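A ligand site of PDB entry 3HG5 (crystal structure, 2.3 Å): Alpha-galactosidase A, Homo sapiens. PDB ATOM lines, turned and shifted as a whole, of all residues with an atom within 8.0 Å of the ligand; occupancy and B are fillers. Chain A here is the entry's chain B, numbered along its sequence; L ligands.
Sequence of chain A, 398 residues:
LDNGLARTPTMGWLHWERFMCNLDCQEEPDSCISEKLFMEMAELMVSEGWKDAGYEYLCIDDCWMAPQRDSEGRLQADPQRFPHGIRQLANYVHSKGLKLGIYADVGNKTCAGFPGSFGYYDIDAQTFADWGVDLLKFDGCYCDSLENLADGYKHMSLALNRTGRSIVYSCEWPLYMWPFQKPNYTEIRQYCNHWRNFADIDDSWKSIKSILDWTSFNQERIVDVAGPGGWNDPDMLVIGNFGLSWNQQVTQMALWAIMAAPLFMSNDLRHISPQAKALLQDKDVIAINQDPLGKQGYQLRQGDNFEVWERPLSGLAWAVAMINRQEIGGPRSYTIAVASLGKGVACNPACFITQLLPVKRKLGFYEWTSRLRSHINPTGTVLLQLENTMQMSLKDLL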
ATOM      1  N   THR A 215      31.911 -22.566   9.980  1.00  0.00           N
ATOM      2  CA  THR A 215      30.847 -21.570   9.966  1.00  0.00           C
ATOM      3  C   THR A 215      30.995 -20.642   8.754  1.00  0.00           C
ATOM      4  O   THR A 215      30.044 -20.440   8.011  1.00  0.00           O
ATOM      5  CB  THR A 215      30.814 -20.755  11.287  1.00  0.00           C
ATOM      6  OG1 THR A 215      30.608 -21.647  12.388  1.00  0.00           O
ATOM      7  CG2 THR A 215      29.715 -19.705  11.269  1.00  0.00           C
ATOM      8  N   SER A 216      32.200 -20.113   8.554  1.00  0.00           N
ATOM      9  CA  SER A 216      32.421 -19.186   7.449  1.00  0.00           C
ATOM     10  C   SER A 216      32.408 -19.907   6.098  1.00  0.00           C
ATOM     11  O   SER A 216      31.987 -19.330   5.085  1.00  0.00           O
ATOM     12  CB  SER A 216      33.697 -18.362   7.637  1.00  0.00           C
ATOM     13  OG  SER A 216      34.849 -19.179   7.579  1.00  0.00           O
ATOM     14  N   ASN A 218      30.415 -22.381   5.455  1.00  0.00           N
ATOM     15  CA  ASN A 218      29.003 -22.712   5.249  1.00  0.00           C
ATOM     16  C   ASN A 218      28.045 -21.532   5.424  1.00  0.00           C
ATOM     17  O   ASN A 218      26.833 -21.730   5.492  1.00  0.00           O
ATOM     18  CB  ASN A 218      28.603 -23.823   6.226  1.00  0.00           C
ATOM     19  CG  ASN A 218      29.202 -25.166   5.874  1.00  0.00           C
ATOM     20  OD1 ASN A 218      28.709 -25.866   4.995  1.00  0.00           O
ATOM     21  ND2 ASN A 218      30.276 -25.544   6.568  1.00  0.00           N
ATOM     22  N   GLN A 219      28.588 -20.317   5.498  1.00  0.00           N
ATOM     23  CA  GLN A 219      27.802 -19.158   5.932  1.00  0.00           C
ATOM     24  C   GLN A 219      26.632 -18.797   5.023  1.00  0.00           C
ATOM     25  O   GLN A 219      25.598 -18.329   5.514  1.00  0.00           O
ATOM     26  CB  GLN A 219      28.703 -17.946   6.218  1.00  0.00           C
ATOM     27  CG  GLN A 219      29.317 -17.240   5.013  1.00  0.00           C
ATOM     28  CD  GLN A 219      30.223 -16.083   5.442  1.00  0.00           C
ATOM     29  OE1 GLN A 219      30.492 -15.900   6.641  1.00  0.00           O
ATOM     30  NE2 GLN A 219      30.698 -15.318   4.469  1.00  0.00           N
ATOM     31  N   GLU A 220      26.796 -19.006   3.721  1.00  0.00           N
ATOM     32  CA  GLU A 220      25.714 -18.785   2.759  1.00  0.00           C
ATOM     33  C   GLU A 220      24.496 -19.664   3.072  1.00  0.00           C
ATOM     34  O   GLU A 220      23.366 -19.303   2.744  1.00  0.00           O
ATOM     35  CB  GLU A 220      26.191 -19.015   1.321  1.00  0.00           C
ATOM     36  CG  GLU A 220      27.034 -17.880   0.701  1.00  0.00           C
ATOM     37  CD  GLU A 220      27.547 -18.221  -0.716  1.00  0.00           C
ATOM     38  OE1 GLU A 220      28.035 -19.358  -0.930  1.00  0.00           O
ATOM     39  OE2 GLU A 220      27.457 -17.365  -1.630  1.00  0.00           O
ATOM     40  N   ARG A 221      24.719 -20.818   3.704  1.00  0.00           N
ATOM     41  CA  ARG A 221      23.642 -21.720   4.105  1.00  0.00           C
ATOM     42  C   ARG A 221      22.936 -21.290   5.388  1.00  0.00           C
ATOM     43  O   ARG A 221      21.718 -21.370   5.485  1.00  0.00           O
ATOM     44  CB  ARG A 221      24.163 -23.155   4.300  1.00  0.00           C
ATOM     45  CG  ARG A 221      24.507 -23.894   3.029  1.00  0.00           C
ATOM     46  CD  ARG A 221      24.863 -25.359   3.298  1.00  0.00           C
ATOM     47  NE  ARG A 221      24.766 -26.142   2.059  1.00  0.00           N
ATOM     48  CZ  ARG A 221      25.771 -26.340   1.206  1.00  0.00           C
ATOM     49  NH1 ARG A 221      26.982 -25.852   1.448  1.00  0.00           N
ATOM     50  NH2 ARG A 221      25.558 -27.056   0.094  1.00  0.00           N
ATOM     51  N   ILE A 222      23.716 -20.846   6.382  1.00  0.00           N
ATOM     52  CA  ILE A 222      23.211 -20.773   7.753  1.00  0.00           C
ATOM     53  C   ILE A 222      22.996 -19.387   8.352  1.00  0.00           C
ATOM     54  O   ILE A 222      22.219 -19.262   9.305  1.00  0.00           O
ATOM     55  CB  ILE A 222      24.080 -21.618   8.748  1.00  0.00           C
ATOM     56  CG1 ILE A 222      25.495 -21.033   8.880  1.00  0.00           C
ATOM     57  CG2 ILE A 222      24.095 -23.086   8.327  1.00  0.00           C
ATOM     58  CD1 ILE A 222      26.242 -21.443  10.141  1.00  0.00           C
ATOM     59  N   VAL A 223      23.668 -18.361   7.830  1.00  0.00           N
ATOM     60  CA  VAL A 223      23.632 -17.025   8.449  1.00  0.00           C
ATOM     61  C   VAL A 223      22.219 -16.454   8.491  1.00  0.00           C
ATOM     62  O   VAL A 223      21.763 -16.037   9.562  1.00  0.00           O
ATOM     63  CB  VAL A 223      24.656 -16.010   7.823  1.00  0.00           C
ATOM     64  CG1 VAL A 223      24.302 -14.565   8.163  1.00  0.00           C
ATOM     65  CG2 VAL A 223      26.072 -16.308   8.297  1.00  0.00           C
ATOM     66  N   ASP A 224      21.536 -16.473   7.352  1.00  0.00           N
ATOM     67  CA  ASP A 224      20.242 -15.798   7.188  1.00  0.00           C
ATOM     68  C   ASP A 224      19.042 -16.519   7.829  1.00  0.00           C
ATOM     69  O   ASP A 224      17.998 -15.878   8.025  1.00  0.00           O
ATOM     70  CB  ASP A 224      19.966 -15.472   5.712  1.00  0.00           C
ATOM     71  CG  ASP A 224      20.903 -14.392   5.156  1.00  0.00           C
ATOM     72  OD1 ASP A 224      21.326 -13.483   5.913  1.00  0.00           O
ATOM     73  OD2 ASP A 224      21.221 -14.457   3.954  1.00  0.00           O
ATOM     74  N   VAL A 225      19.174 -17.809   8.127  1.00  0.00           N
ATOM     75  CA  VAL A 225      18.114 -18.548   8.827  1.00  0.00           C
ATOM     76  C   VAL A 225      18.053 -18.196  10.312  1.00  0.00           C
ATOM     77  O   VAL A 225      17.010 -18.359  10.972  1.00  0.00           O
ATOM     78  CB  VAL A 225      18.168 -20.101   8.624  1.00  0.00           C
ATOM     79  CG1 VAL A 225      17.989 -20.468   7.150  1.00  0.00           C
ATOM     80  CG2 VAL A 225      19.442 -20.691   9.131  1.00  0.00           C
ATOM     81  N   LYS A 295      20.222 -10.402  14.107  1.00  0.00           N
ATOM     82  CA  LYS A 295      20.773 -10.708  12.794  1.00  0.00           C
ATOM     83  C   LYS A 295      22.197 -11.234  12.972  1.00  0.00           C
ATOM     84  O   LYS A 295      23.042 -10.538  13.549  1.00  0.00           O
ATOM     85  CB  LYS A 295      20.746  -9.444  11.939  1.00  0.00           C
ATOM     86  CG  LYS A 295      21.057  -9.659  10.478  1.00  0.00           C
ATOM     87  CD  LYS A 295      20.635  -8.441   9.667  1.00  0.00           C
ATOM     88  CE  LYS A 295      19.431  -8.708   8.802  1.00  0.00           C
ATOM     89  NZ  LYS A 295      19.812  -9.596   7.672  1.00  0.00           N
ATOM     90  N   GLN A 296      22.444 -12.451  12.507  1.00  0.00           N
ATOM     91  CA  GLN A 296      23.755 -13.087  12.674  1.00  0.00           C
ATOM     92  C   GLN A 296      24.787 -12.432  11.750  1.00  0.00           C
ATOM     93  O   GLN A 296      24.467 -12.066  10.619  1.00  0.00           O
ATOM     94  CB  GLN A 296      23.681 -14.604  12.421  1.00  0.00           C
ATOM     95  CG  GLN A 296      25.048 -15.305  12.401  1.00  0.00           C
ATOM     96  CD  GLN A 296      24.985 -16.825  12.547  1.00  0.00           C
ATOM     97  OE1 GLN A 296      23.961 -17.383  12.956  1.00  0.00           O
ATOM     98  NE2 GLN A 296      26.080 -17.501  12.219  1.00  0.00           N
ATOM     99  N   GLY A 297      26.009 -12.291  12.251  1.00  0.00           N
ATOM    100  CA  GLY A 297      27.123 -11.759  11.471  1.00  0.00           C
ATOM    101  C   GLY A 297      27.760 -12.789  10.560  1.00  0.00           C
ATOM    102  O   GLY A 297      27.296 -13.916  10.460  1.00  0.00           O
ATOM    103  N   TYR A 298      28.847 -12.391   9.902  1.00  0.00           N
ATOM    104  CA  TYR A 298      29.414 -13.195   8.818  1.00  0.00           C
ATOM    105  C   TYR A 298      30.852 -12.795   8.590  1.00  0.00           C
ATOM    106  O   TYR A 298      31.304 -11.756   9.071  1.00  0.00           O
ATOM    107  CB  TYR A 298      28.595 -12.997   7.532  1.00  0.00           C
ATOM    108  CG  TYR A 298      28.433 -11.534   7.138  1.00  0.00           C
ATOM    109  CD1 TYR A 298      29.400 -10.890   6.359  1.00  0.00           C
ATOM    110  CD2 TYR A 298      27.326 -10.802   7.571  1.00  0.00           C
ATOM    111  CE1 TYR A 298      29.268  -9.549   6.022  1.00  0.00           C
ATOM    112  CE2 TYR A 298      27.188  -9.449   7.239  1.00  0.00           C
ATOM    113  CZ  TYR A 298      28.156  -8.834   6.468  1.00  0.00           C
ATOM    114  OH  TYR A 298      28.029  -7.505   6.126  1.00  0.00           O
ATOM    115  N   GLN A 299      31.590 -13.624   7.844  1.00  0.00           N
ATOM    116  CA  GLN A 299      32.939 -13.269   7.433  1.00  0.00           C
ATOM    117  C   GLN A 299      32.908 -12.379   6.190  1.00  0.00           C
ATOM    118  O   GLN A 299      32.371 -12.750   5.154  1.00  0.00           O
ATOM    119  CB  GLN A 299      33.764 -14.526   7.138  1.00  0.00           C
ATOM    120  CG  GLN A 299      35.262 -14.257   7.106  1.00  0.00           C
ATOM    121  CD  GLN A 299      36.027 -15.357   6.415  1.00  0.00           C
ATOM    122  OE1 GLN A 299      35.815 -15.612   5.227  1.00  0.00           O
ATOM    123  NE2 GLN A 299      36.931 -16.014   7.141  1.00  0.00           N
ATOM    124  N   LEU A 300      33.494 -11.188   6.320  1.00  0.00           N
ATOM    125  CA  LEU A 300      33.558 -10.217   5.244  1.00  0.00           C
ATOM    126  C   LEU A 300      34.768 -10.486   4.353  1.00  0.00           C
ATOM    127  O   LEU A 300      34.643 -10.468   3.126  1.00  0.00           O
ATOM    128  CB  LEU A 300      33.601  -8.788   5.807  1.00  0.00           C
ATOM    129  CG  LEU A 300      33.807  -7.621   4.834  1.00  0.00           C
ATOM    130  CD1 LEU A 300      32.588  -7.413   3.940  1.00  0.00           C
ATOM    131  CD2 LEU A 300      34.156  -6.332   5.586  1.00  0.00           C
ATOM    132  N   GLU A 310      31.898  -9.123  10.449  1.00  0.00           N
ATOM    133  CA  GLU A 310      31.070  -8.007  10.904  1.00  0.00           C
ATOM    134  C   GLU A 310      29.652  -8.464  11.220  1.00  0.00           C
ATOM    135  O   GLU A 310      29.225  -9.534  10.754  1.00  0.00           O
ATOM    136  CB  GLU A 310      31.072  -6.840   9.906  1.00  0.00           C
ATOM    137  CG  GLU A 310      30.404  -7.114   8.555  1.00  0.00           C
ATOM    138  CD  GLU A 310      30.604  -5.975   7.567  1.00  0.00           C
ATOM    139  OE1 GLU A 310      31.376  -5.045   7.874  1.00  0.00           O
ATOM    140  OE2 GLU A 310      29.985  -5.997   6.475  1.00  0.00           O
ATOM    141  N   PRO A 312      25.600  -6.719  11.652  1.00  0.00           N
ATOM    142  CA  PRO A 312      24.676  -5.583  11.773  1.00  0.00           C
ATOM    143  C   PRO A 312      23.891  -5.628  13.089  1.00  0.00           C
ATOM    144  O   PRO A 312      23.349  -6.676  13.470  1.00  0.00           O
ATOM    145  CB  PRO A 312      23.752  -5.746  10.561  1.00  0.00           C
ATOM    146  CG  PRO A 312      23.840  -7.189  10.187  1.00  0.00           C
ATOM    147  CD  PRO A 312      25.152  -7.713  10.658  1.00  0.00           C
ATOM    148  N   TRP A 318      27.225  -1.298  13.947  1.00  0.00           N
ATOM    149  CA  TRP A 318      27.904  -2.531  13.539  1.00  0.00           C
ATOM    150  C   TRP A 318      28.959  -2.953  14.530  1.00  0.00           C
ATOM    151  O   TRP A 318      29.624  -2.124  15.142  1.00  0.00           O
ATOM    152  CB  TRP A 318      28.562  -2.370  12.162  1.00  0.00           C
ATOM    153  CG  TRP A 318      27.695  -2.836  11.043  1.00  0.00           C
ATOM    154  CD1 TRP A 318      27.720  -4.067  10.440  1.00  0.00           C
ATOM    155  CD2 TRP A 318      26.669  -2.078  10.383  1.00  0.00           C
ATOM    156  NE1 TRP A 318      26.781  -4.120   9.447  1.00  0.00           N
ATOM    157  CE2 TRP A 318      26.120  -2.922   9.385  1.00  0.00           C
ATOM    158  CE3 TRP A 318      26.161  -0.791  10.542  1.00  0.00           C
ATOM    159  CZ2 TRP A 318      25.090  -2.510   8.548  1.00  0.00           C
ATOM    160  CZ3 TRP A 318      25.137  -0.373   9.698  1.00  0.00           C
ATOM    161  CH2 TRP A 318      24.599  -1.229   8.719  1.00  0.00           C
ATOM    162  N   LYS A 343      28.571  -2.591   4.883  1.00  0.00           N
ATOM    163  CA  LYS A 343      28.064  -2.377   3.525  1.00  0.00           C
ATOM    164  C   LYS A 343      28.028  -0.904   3.135  1.00  0.00           C
ATOM    165  O   LYS A 343      27.127  -0.455   2.411  1.00  0.00           O
ATOM    166  CB  LYS A 343      26.684  -3.016   3.346  1.00  0.00           C
ATOM    167  CG  LYS A 343      26.699  -4.529   3.475  1.00  0.00           C
ATOM    168  CD  LYS A 343      25.305  -5.077   3.684  1.00  0.00           C
ATOM    169  CE  LYS A 343      25.349  -6.502   4.177  1.00  0.00           C
ATOM    170  NZ  LYS A 343      26.156  -7.378   3.290  1.00  0.00           N
HETATM  171  C1  LIG L   1      26.359 -11.018   3.685  1.00  0.00           C
HETATM  172  C2  LIG L   1      24.854 -10.814   3.879  1.00  0.00           C
HETATM  173  C3  LIG L   1      24.296 -11.834   4.877  1.00  0.00           C
HETATM  174  C4  LIG L   1      24.696 -13.260   4.483  1.00  0.00           C
HETATM  175  C5  LIG L   1      26.212 -13.327   4.272  1.00  0.00           C
HETATM  176  C6  LIG L   1      26.711 -14.723   3.888  1.00  0.00           C
HETATM  177  O1  LIG L   1      26.901 -10.130   2.688  1.00  0.00           O
HETATM  178  O2  LIG L   1      24.552  -9.491   4.333  1.00  0.00           O
HETATM  179  O3  LIG L   1      22.868 -11.735   4.971  1.00  0.00           O
HETATM  180  O4  LIG L   1      23.967 -13.625   3.309  1.00  0.00           O
HETATM  181  O5  LIG L   1      26.623 -12.367   3.289  1.00  0.00           O
HETATM  182  O6  LIG L   1      27.838 -14.634   3.011  1.00  0.00           O
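An oxygen (O3) of the ligand lies within hydrogen-bond range of the side-chain carboxylate (OD1) of Asp 224, 2.5 Å away.
O2 of the ligand sits at hydrogen-bond distance from NZ of Lys 343.
The side-chain amide nitrogen (NE2) of Gln 219 lies within hydrogen-bond range of an oxygen (O6) of the ligand (3.3 Å).
The side-chain carboxylate (OE2) of Glu 310 sits at hydrogen-bond distance from the side-chain hydroxyl (OH) of Tyr 298.
The side-chain amino group (NZ) of Lys 343 lies within hydrogen-bond range of the side-chain hydroxyl (OH) of Tyr 298 (3.4 Å).
The backbone NH of Gln 299 lies within hydrogen-bond range of the side-chain amide oxygen of Gln 219 (2.8 Å).
Merely in contact with the ligand: Val 223 (3.9 Å) and Tyr 298 (3.9 Å).
Hydrophobic or aromatic side chains that line the ligand: Val 223 and Tyr 298.
Five residues have an atom within 4 Å of the ligand: Gln 219, Val 223, Asp 224, Tyr 298 and Lys 343.
The nearest printed residue that does not touch the ligand is Glu 220 (4.1 Å).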
